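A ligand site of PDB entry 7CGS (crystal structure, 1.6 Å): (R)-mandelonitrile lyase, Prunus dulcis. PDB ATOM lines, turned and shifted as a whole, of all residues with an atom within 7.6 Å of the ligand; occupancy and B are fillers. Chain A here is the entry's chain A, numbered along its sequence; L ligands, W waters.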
ATOM      1  N   LYS A 158     -22.695  -9.985  18.839  1.00  0.00           N
ATOM      2  CA  LYS A 158     -21.473 -10.687  18.402  1.00  0.00           C
ATOM      3  C   LYS A 158     -20.754  -9.790  17.399  1.00  0.00           C
ATOM      4  O   LYS A 158     -21.313  -9.466  16.339  1.00  0.00           O
ATOM      5  CB  LYS A 158     -21.853 -11.973  17.679  1.00  0.00           C
ATOM      6  CG  LYS A 158     -20.659 -12.747  17.169  1.00  0.00           C
ATOM      7  CD  LYS A 158     -21.140 -13.928  16.299  1.00  0.00           C
ATOM      8  CE  LYS A 158     -20.130 -15.040  16.202  1.00  0.00           C
ATOM      9  NZ  LYS A 158     -18.860 -14.515  15.708  1.00  0.00           N
ATOM     10  N   PRO A 159     -19.531  -9.293  17.707  1.00  0.00           N
ATOM     11  CA  PRO A 159     -18.825  -8.394  16.799  1.00  0.00           C
ATOM     12  C   PRO A 159     -18.485  -9.066  15.453  1.00  0.00           C
ATOM     13  O   PRO A 159     -18.178 -10.234  15.418  1.00  0.00           O
ATOM     14  CB  PRO A 159     -17.528  -8.030  17.552  1.00  0.00           C
ATOM     15  CG  PRO A 159     -17.862  -8.345  18.966  1.00  0.00           C
ATOM     16  CD  PRO A 159     -18.778  -9.524  18.943  1.00  0.00           C
ATOM     17  N   ASN A 160     -18.536  -8.258  14.412  1.00  0.00           N
ATOM     18  CA  ASN A 160     -17.948  -8.615  13.101  1.00  0.00           C
ATOM     19  C   ASN A 160     -16.417  -8.659  13.237  1.00  0.00           C
ATOM     20  O   ASN A 160     -15.818  -8.056  14.185  1.00  0.00           O
ATOM     21  CB  ASN A 160     -18.437  -7.643  12.029  1.00  0.00           C
ATOM     22  CG  ASN A 160     -19.818  -7.966  11.532  1.00  0.00           C
ATOM     23  OD1 ASN A 160     -20.334  -9.044  11.840  1.00  0.00           O
ATOM     24  ND2 ASN A 160     -20.435  -7.024  10.814  1.00  0.00           N
ATOM     25  N   ASN A 161     -15.804  -9.277  12.245  1.00  0.00           N
ATOM     26  CA  ASN A 161     -14.318  -9.311  12.112  1.00  0.00           C
ATOM     27  C   ASN A 161     -13.775  -7.902  11.995  1.00  0.00           C
ATOM     28  O   ASN A 161     -14.349  -7.069  11.243  1.00  0.00           O
ATOM     29  CB  ASN A 161     -13.881  -9.987  10.810  1.00  0.00           C
ATOM     30  CG  ASN A 161     -14.154 -11.456  10.770  1.00  0.00           C
ATOM     31  OD1 ASN A 161     -13.913 -12.157  11.747  1.00  0.00           O
ATOM     32  ND2 ASN A 161     -14.572 -11.924   9.602  1.00  0.00           N
ATOM     33  N   GLN A 162     -12.688  -7.632  12.689  1.00  0.00           N
ATOM     34  CA  GLN A 162     -11.893  -6.398  12.545  1.00  0.00           C
ATOM     35  C   GLN A 162     -10.448  -6.839  12.368  1.00  0.00           C
ATOM     36  O   GLN A 162      -9.966  -7.625  13.180  1.00  0.00           O
ATOM     37  CB  GLN A 162     -12.008  -5.520  13.795  1.00  0.00           C
ATOM     38  CG  GLN A 162     -13.438  -4.990  14.047  1.00  0.00           C
ATOM     39  CD  GLN A 162     -13.490  -4.260  15.360  1.00  0.00           C
ATOM     40  OE1 GLN A 162     -13.440  -3.024  15.368  1.00  0.00           O
ATOM     41  NE2 GLN A 162     -13.521  -5.016  16.453  1.00  0.00           N
ATOM     42  N   GLN A 165      -8.060  -6.656  15.465  1.00  0.00           N
ATOM     43  CA  GLN A 165      -8.452  -7.589  16.532  1.00  0.00           C
ATOM     44  C   GLN A 165      -8.094  -9.033  16.137  1.00  0.00           C
ATOM     45  O   GLN A 165      -7.672  -9.777  17.002  1.00  0.00           O
ATOM     46  CB  GLN A 165      -9.932  -7.444  16.864  1.00  0.00           C
ATOM     47  CG  GLN A 165     -10.331  -6.038  17.338  1.00  0.00           C
ATOM     48  CD  GLN A 165      -9.628  -5.690  18.638  1.00  0.00           C
ATOM     49  OE1 GLN A 165      -9.646  -6.448  19.637  1.00  0.00           O
ATOM     50  NE2 GLN A 165      -8.899  -4.601  18.600  1.00  0.00           N
ATOM     51  N   SER A 166      -8.211  -9.390  14.873  1.00  0.00           N
ATOM     52  CA  SER A 166      -7.832 -10.731  14.374  1.00  0.00           C
ATOM     53  C   SER A 166      -6.323 -10.930  14.471  1.00  0.00           C
ATOM     54  O   SER A 166      -5.881 -11.986  14.949  1.00  0.00           O
ATOM     55  CB  SER A 166      -8.376 -10.889  13.032  1.00  0.00           C
ATOM     56  OG  SER A 166      -9.796 -11.035  13.113  1.00  0.00           O
ATOM     57  N   VAL A 167      -5.536  -9.930  14.121  1.00  0.00           N
ATOM     58  CA  VAL A 167      -4.068 -10.008  14.249  1.00  0.00           C
ATOM     59  C   VAL A 167      -3.695 -10.273  15.705  1.00  0.00           C
ATOM     60  O   VAL A 167      -2.896 -11.167  16.012  1.00  0.00           O
ATOM     61  CB  VAL A 167      -3.414  -8.716  13.750  1.00  0.00           C
ATOM     62  CG1 VAL A 167      -1.978  -8.602  14.231  1.00  0.00           C
ATOM     63  CG2 VAL A 167      -3.538  -8.534  12.243  1.00  0.00           C
ATOM     64  N   ILE A 168      -4.275  -9.493  16.618  1.00  0.00           N
ATOM     65  CA  ILE A 168      -3.910  -9.623  18.039  1.00  0.00           C
ATOM     66  C   ILE A 168      -4.336 -11.007  18.549  1.00  0.00           C
ATOM     67  O   ILE A 168      -3.592 -11.585  19.370  1.00  0.00           O
ATOM     68  CB  ILE A 168      -4.529  -8.438  18.794  1.00  0.00           C
ATOM     69  CG1 ILE A 168      -3.699  -7.193  18.528  1.00  0.00           C
ATOM     70  CG2 ILE A 168      -4.610  -8.721  20.245  1.00  0.00           C
ATOM     71  CD1 ILE A 168      -2.314  -7.201  19.240  1.00  0.00           C
ATOM     72  N   GLY A 169      -5.482 -11.511  18.108  1.00  0.00           N
ATOM     73  CA  GLY A 169      -5.936 -12.830  18.579  1.00  0.00           C
ATOM     74  C   GLY A 169      -4.981 -13.909  18.069  1.00  0.00           C
ATOM     75  O   GLY A 169      -4.629 -14.814  18.842  1.00  0.00           O
ATOM     76  N   GLU A 170      -4.557 -13.789  16.819  1.00  0.00           N
ATOM     77  CA  GLU A 170      -3.562 -14.782  16.296  1.00  0.00           C
ATOM     78  C   GLU A 170      -2.285 -14.669  17.099  1.00  0.00           C
ATOM     79  O   GLU A 170      -1.651 -15.714  17.402  1.00  0.00           O
ATOM     80  CB  GLU A 170      -3.263 -14.551  14.819  1.00  0.00           C
ATOM     81  CG  GLU A 170      -4.423 -14.851  13.888  1.00  0.00           C
ATOM     82  CD  GLU A 170      -5.039 -16.243  13.980  1.00  0.00           C
ATOM     83  OE1 GLU A 170      -4.368 -17.185  14.432  1.00  0.00           O
ATOM     84  OE2 GLU A 170      -6.207 -16.362  13.596  1.00  0.00           O
ATOM     85  N   GLY A 171      -1.864 -13.453  17.466  1.00  0.00           N
ATOM     86  CA  GLY A 171      -0.677 -13.218  18.290  1.00  0.00           C
ATOM     87  C   GLY A 171      -0.818 -13.813  19.677  1.00  0.00           C
ATOM     88  O   GLY A 171       0.119 -14.454  20.185  1.00  0.00           O
ATOM     89  N   LEU A 173      -2.632 -16.295  20.641  1.00  0.00           N
ATOM     90  CA  LEU A 173      -2.601 -17.790  20.517  1.00  0.00           C
ATOM     91  C   LEU A 173      -1.169 -18.225  20.266  1.00  0.00           C
ATOM     92  O   LEU A 173      -0.715 -19.149  20.953  1.00  0.00           O
ATOM     93  CB  LEU A 173      -3.542 -18.225  19.401  1.00  0.00           C
ATOM     94  CG  LEU A 173      -5.021 -18.111  19.775  1.00  0.00           C
ATOM     95  CD1 LEU A 173      -5.900 -18.237  18.568  1.00  0.00           C
ATOM     96  CD2 LEU A 173      -5.398 -19.096  20.848  1.00  0.00           C
ATOM     97  N   PRO A 179      -6.600 -22.007  25.727  1.00  0.00           N
ATOM     98  CA  PRO A 179      -6.879 -22.403  24.346  1.00  0.00           C
ATOM     99  C   PRO A 179      -7.585 -21.321  23.533  1.00  0.00           C
ATOM    100  O   PRO A 179      -7.854 -20.252  24.100  1.00  0.00           O
ATOM    101  CB  PRO A 179      -7.836 -23.578  24.583  1.00  0.00           C
ATOM    102  CG  PRO A 179      -8.609 -23.178  25.814  1.00  0.00           C
ATOM    103  CD  PRO A 179      -7.608 -22.479  26.681  1.00  0.00           C
ATOM    104  N   ASP A 180      -7.940 -21.636  22.300  1.00  0.00           N
ATOM    105  CA  ASP A 180      -8.718 -20.779  21.453  1.00  0.00           C
ATOM    106  C   ASP A 180     -10.150 -21.052  21.782  1.00  0.00           C
ATOM    107  O   ASP A 180     -10.681 -22.174  21.557  1.00  0.00           O
ATOM    108  CB  ASP A 180      -8.403 -21.119  19.973  1.00  0.00           C
ATOM    109  CG  ASP A 180      -9.112 -20.239  18.983  1.00  0.00           C
ATOM    110  OD1 ASP A 180     -10.027 -19.444  19.353  1.00  0.00           O
ATOM    111  OD2 ASP A 180      -8.822 -20.387  17.770  1.00  0.00           O
ATOM    112  N   ASN A 181     -10.815 -20.071  22.386  1.00  0.00           N
ATOM    113  CA  ASN A 181     -12.225 -20.192  22.823  1.00  0.00           C
ATOM    114  C   ASN A 181     -13.193 -19.693  21.742  1.00  0.00           C
ATOM    115  O   ASN A 181     -14.405 -19.702  22.016  1.00  0.00           O
ATOM    116  CB  ASN A 181     -12.454 -19.451  24.134  1.00  0.00           C
ATOM    117  CG  ASN A 181     -11.627 -20.033  25.262  1.00  0.00           C
ATOM    118  OD1 ASN A 181     -11.528 -21.264  25.373  1.00  0.00           O
ATOM    119  ND2 ASN A 181     -11.051 -19.188  26.097  1.00  0.00           N
ATOM    120  N   GLY A 182     -12.728 -19.261  20.581  1.00  0.00           N
ATOM    121  CA  GLY A 182     -13.654 -18.799  19.550  1.00  0.00           C
ATOM    122  C   GLY A 182     -14.459 -17.601  20.019  1.00  0.00           C
ATOM    123  O   GLY A 182     -13.878 -16.745  20.697  1.00  0.00           O
ATOM    124  N   PHE A 183     -15.725 -17.495  19.615  1.00  0.00           N
ATOM    125  CA  PHE A 183     -16.632 -16.446  20.131  1.00  0.00           C
ATOM    126  C   PHE A 183     -17.273 -16.942  21.419  1.00  0.00           C
ATOM    127  O   PHE A 183     -17.945 -17.999  21.442  1.00  0.00           O
ATOM    128  CB  PHE A 183     -17.689 -16.051  19.114  1.00  0.00           C
ATOM    129  CG  PHE A 183     -18.740 -15.154  19.702  1.00  0.00           C
ATOM    130  CD1 PHE A 183     -18.398 -13.931  20.255  1.00  0.00           C
ATOM    131  CD2 PHE A 183     -20.075 -15.545  19.710  1.00  0.00           C
ATOM    132  CE1 PHE A 183     -19.358 -13.101  20.799  1.00  0.00           C
ATOM    133  CE2 PHE A 183     -21.037 -14.724  20.289  1.00  0.00           C
ATOM    134  CZ  PHE A 183     -20.669 -13.508  20.822  1.00  0.00           C
ATOM    135  N   THR A 191      -7.792 -17.318  24.561  1.00  0.00           N
ATOM    136  CA  THR A 191      -8.027 -16.208  23.602  1.00  0.00           C
ATOM    137  C   THR A 191      -9.420 -16.335  23.042  1.00  0.00           C
ATOM    138  O   THR A 191      -9.810 -17.442  22.618  1.00  0.00           O
ATOM    139  CB  THR A 191      -6.966 -16.187  22.476  1.00  0.00           C
ATOM    140  OG1 THR A 191      -5.721 -16.024  23.142  1.00  0.00           O
ATOM    141  CG2 THR A 191      -7.219 -15.069  21.507  1.00  0.00           C
ATOM    142  N   ARG A 192     -10.161 -15.238  22.947  1.00  0.00           N
ATOM    143  CA  ARG A 192     -11.520 -15.276  22.437  1.00  0.00           C
ATOM    144  C   ARG A 192     -11.906 -13.954  21.820  1.00  0.00           C
ATOM    145  O   ARG A 192     -11.310 -12.919  22.172  1.00  0.00           O
ATOM    146  CB  ARG A 192     -12.546 -15.647  23.504  1.00  0.00           C
ATOM    147  CG  ARG A 192     -12.937 -14.486  24.421  1.00  0.00           C
ATOM    148  CD  ARG A 192     -13.853 -14.964  25.495  1.00  0.00           C
ATOM    149  NE  ARG A 192     -14.520 -13.935  26.266  1.00  0.00           N
ATOM    150  CZ  ARG A 192     -14.048 -13.325  27.335  1.00  0.00           C
ATOM    151  NH1 ARG A 192     -12.848 -13.628  27.801  1.00  0.00           N
ATOM    152  NH2 ARG A 192     -14.804 -12.413  27.949  1.00  0.00           N
ATOM    153  N   LEU A 193     -12.928 -14.013  20.970  1.00  0.00           N
ATOM    154  CA  LEU A 193     -13.775 -12.870  20.573  1.00  0.00           C
ATOM    155  C   LEU A 193     -14.898 -12.804  21.618  1.00  0.00           C
ATOM    156  O   LEU A 193     -15.599 -13.815  21.817  1.00  0.00           O
ATOM    157  CB  LEU A 193     -14.378 -13.109  19.202  1.00  0.00           C
ATOM    158  CG  LEU A 193     -15.242 -11.979  18.655  1.00  0.00           C
ATOM    159  CD1 LEU A 193     -14.391 -10.796  18.245  1.00  0.00           C
ATOM    160  CD2 LEU A 193     -16.091 -12.471  17.515  1.00  0.00           C
ATOM    161  N   THR A 194     -15.085 -11.656  22.280  1.00  0.00           N
ATOM    162  CA  THR A 194     -16.150 -11.490  23.292  1.00  0.00           C
ATOM    163  C   THR A 194     -17.246 -10.603  22.679  1.00  0.00           C
ATOM    164  O   THR A 194     -17.133 -10.152  21.503  1.00  0.00           O
ATOM    165  CB  THR A 194     -15.583 -10.966  24.625  1.00  0.00           C
ATOM    166  OG1 THR A 194     -16.570 -11.273  25.639  1.00  0.00           O
ATOM    167  CG2 THR A 194     -15.206  -9.517  24.570  1.00  0.00           C
ATOM    168  N   THR A 328     -12.367  -6.239  20.962  1.00  0.00           N
ATOM    169  CA  THR A 328     -13.257  -7.411  20.971  1.00  0.00           C
ATOM    170  C   THR A 328     -12.533  -8.713  21.274  1.00  0.00           C
ATOM    171  O   THR A 328     -13.185  -9.667  21.616  1.00  0.00           O
ATOM    172  CB  THR A 328     -14.025  -7.545  19.659  1.00  0.00           C
ATOM    173  OG1 THR A 328     -13.026  -7.742  18.648  1.00  0.00           O
ATOM    174  CG2 THR A 328     -14.937  -6.362  19.347  1.00  0.00           C
ATOM    175  N   VAL A 329     -11.203  -8.729  21.125  1.00  0.00           N
ATOM    176  CA  VAL A 329     -10.405  -9.956  21.253  1.00  0.00           C
ATOM    177  C   VAL A 329      -9.579  -9.882  22.526  1.00  0.00           C
ATOM    178  O   VAL A 329      -8.754  -8.991  22.689  1.00  0.00           O
ATOM    179  CB  VAL A 329      -9.586 -10.259  19.997  1.00  0.00           C
ATOM    180  CG1 VAL A 329      -8.612 -11.389  20.257  1.00  0.00           C
ATOM    181  CG2 VAL A 329     -10.470 -10.588  18.836  1.00  0.00           C
ATOM    182  N   LEU A 330      -9.806 -10.840  23.436  1.00  0.00           N
ATOM    183  CA  LEU A 330      -9.205 -10.867  24.780  1.00  0.00           C
ATOM    184  C   LEU A 330      -8.269 -12.064  24.939  1.00  0.00           C
ATOM    185  O   LEU A 330      -8.648 -13.191  24.536  1.00  0.00           O
ATOM    186  CB  LEU A 330     -10.350 -10.957  25.784  1.00  0.00           C
ATOM    187  CG  LEU A 330     -11.065  -9.671  26.182  1.00  0.00           C
ATOM    188  CD1 LEU A 330     -11.495  -8.815  25.042  1.00  0.00           C
ATOM    189  CD2 LEU A 330     -12.231  -9.987  27.108  1.00  0.00           C
HETATM  190  N1  LIG L   1     -10.367 -14.688  16.545  1.00  0.00           N
HETATM  191  C1  LIG L   1     -10.432 -15.526  17.676  1.00  0.00           C
HETATM  192  C2  LIG L   1     -10.476 -16.880  16.871  1.00  0.00           C
HETATM  193  O1  LIG L   1     -10.545 -17.582  17.890  1.00  0.00           O
HETATM  194  O2  LIG L   1     -10.506 -17.102  15.502  1.00  0.00           O
HETATM  195  C3  LIG L   1      -9.081 -14.010  16.592  1.00  0.00           C
HETATM  196  C4  LIG L   1      -8.067 -14.711  15.729  1.00  0.00           C
HETATM  197  O3  LIG L   1      -8.508 -15.845  15.021  1.00  0.00           O
HETATM  198  C5  LIG L   1     -11.485 -13.797  16.266  1.00  0.00           C
HETATM  199  C6  LIG L   1     -12.727 -14.524  15.624  1.00  0.00           C
HETATM  200  O4  LIG L   1     -12.334 -15.878  15.481  1.00  0.00           O
HETATM  201  O   HOH W   1      -8.705 -18.777  15.674  1.00  0.00           O
HETATM  202  O   HOH W   2     -13.618 -11.905  14.421  1.00  0.00           O
HETATM  203  O   HOH W   3     -11.746 -19.176  15.471  1.00  0.00           O
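The side-chain carboxylate (OE2) of Glu 170 lies within hydrogen-bond range of an oxygen (O3) of the ligand, at 2.8 Å. OD1 of Asp 180 lies close to O1 of the ligand (2.4 Å).
The side-chain carboxylate (OD1) of Asp 180 lies within hydrogen-bond range of the backbone NH (N) of Gly 182, 3.0 Å away. The side-chain hydroxyl of Ser 166 lies within hydrogen-bond range of the backbone carbonyl oxygen of Gln 162 (3.4 Å). The backbone carbonyl oxygen of Gly 182 sits at hydrogen-bond distance from the backbone NH of Leu 193 (2.9 Å).
Ser 166 touches the ligand. Gly 169 touches the ligand. Gly 182 touches the ligand. Of the 25 residues printed, 5 come within 4 Å of the ligand.
Water W1 bridges an oxygen (O2) of the ligand (2.5 Å) and the side-chain carboxylate of Asp 180 (2.6 Å).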
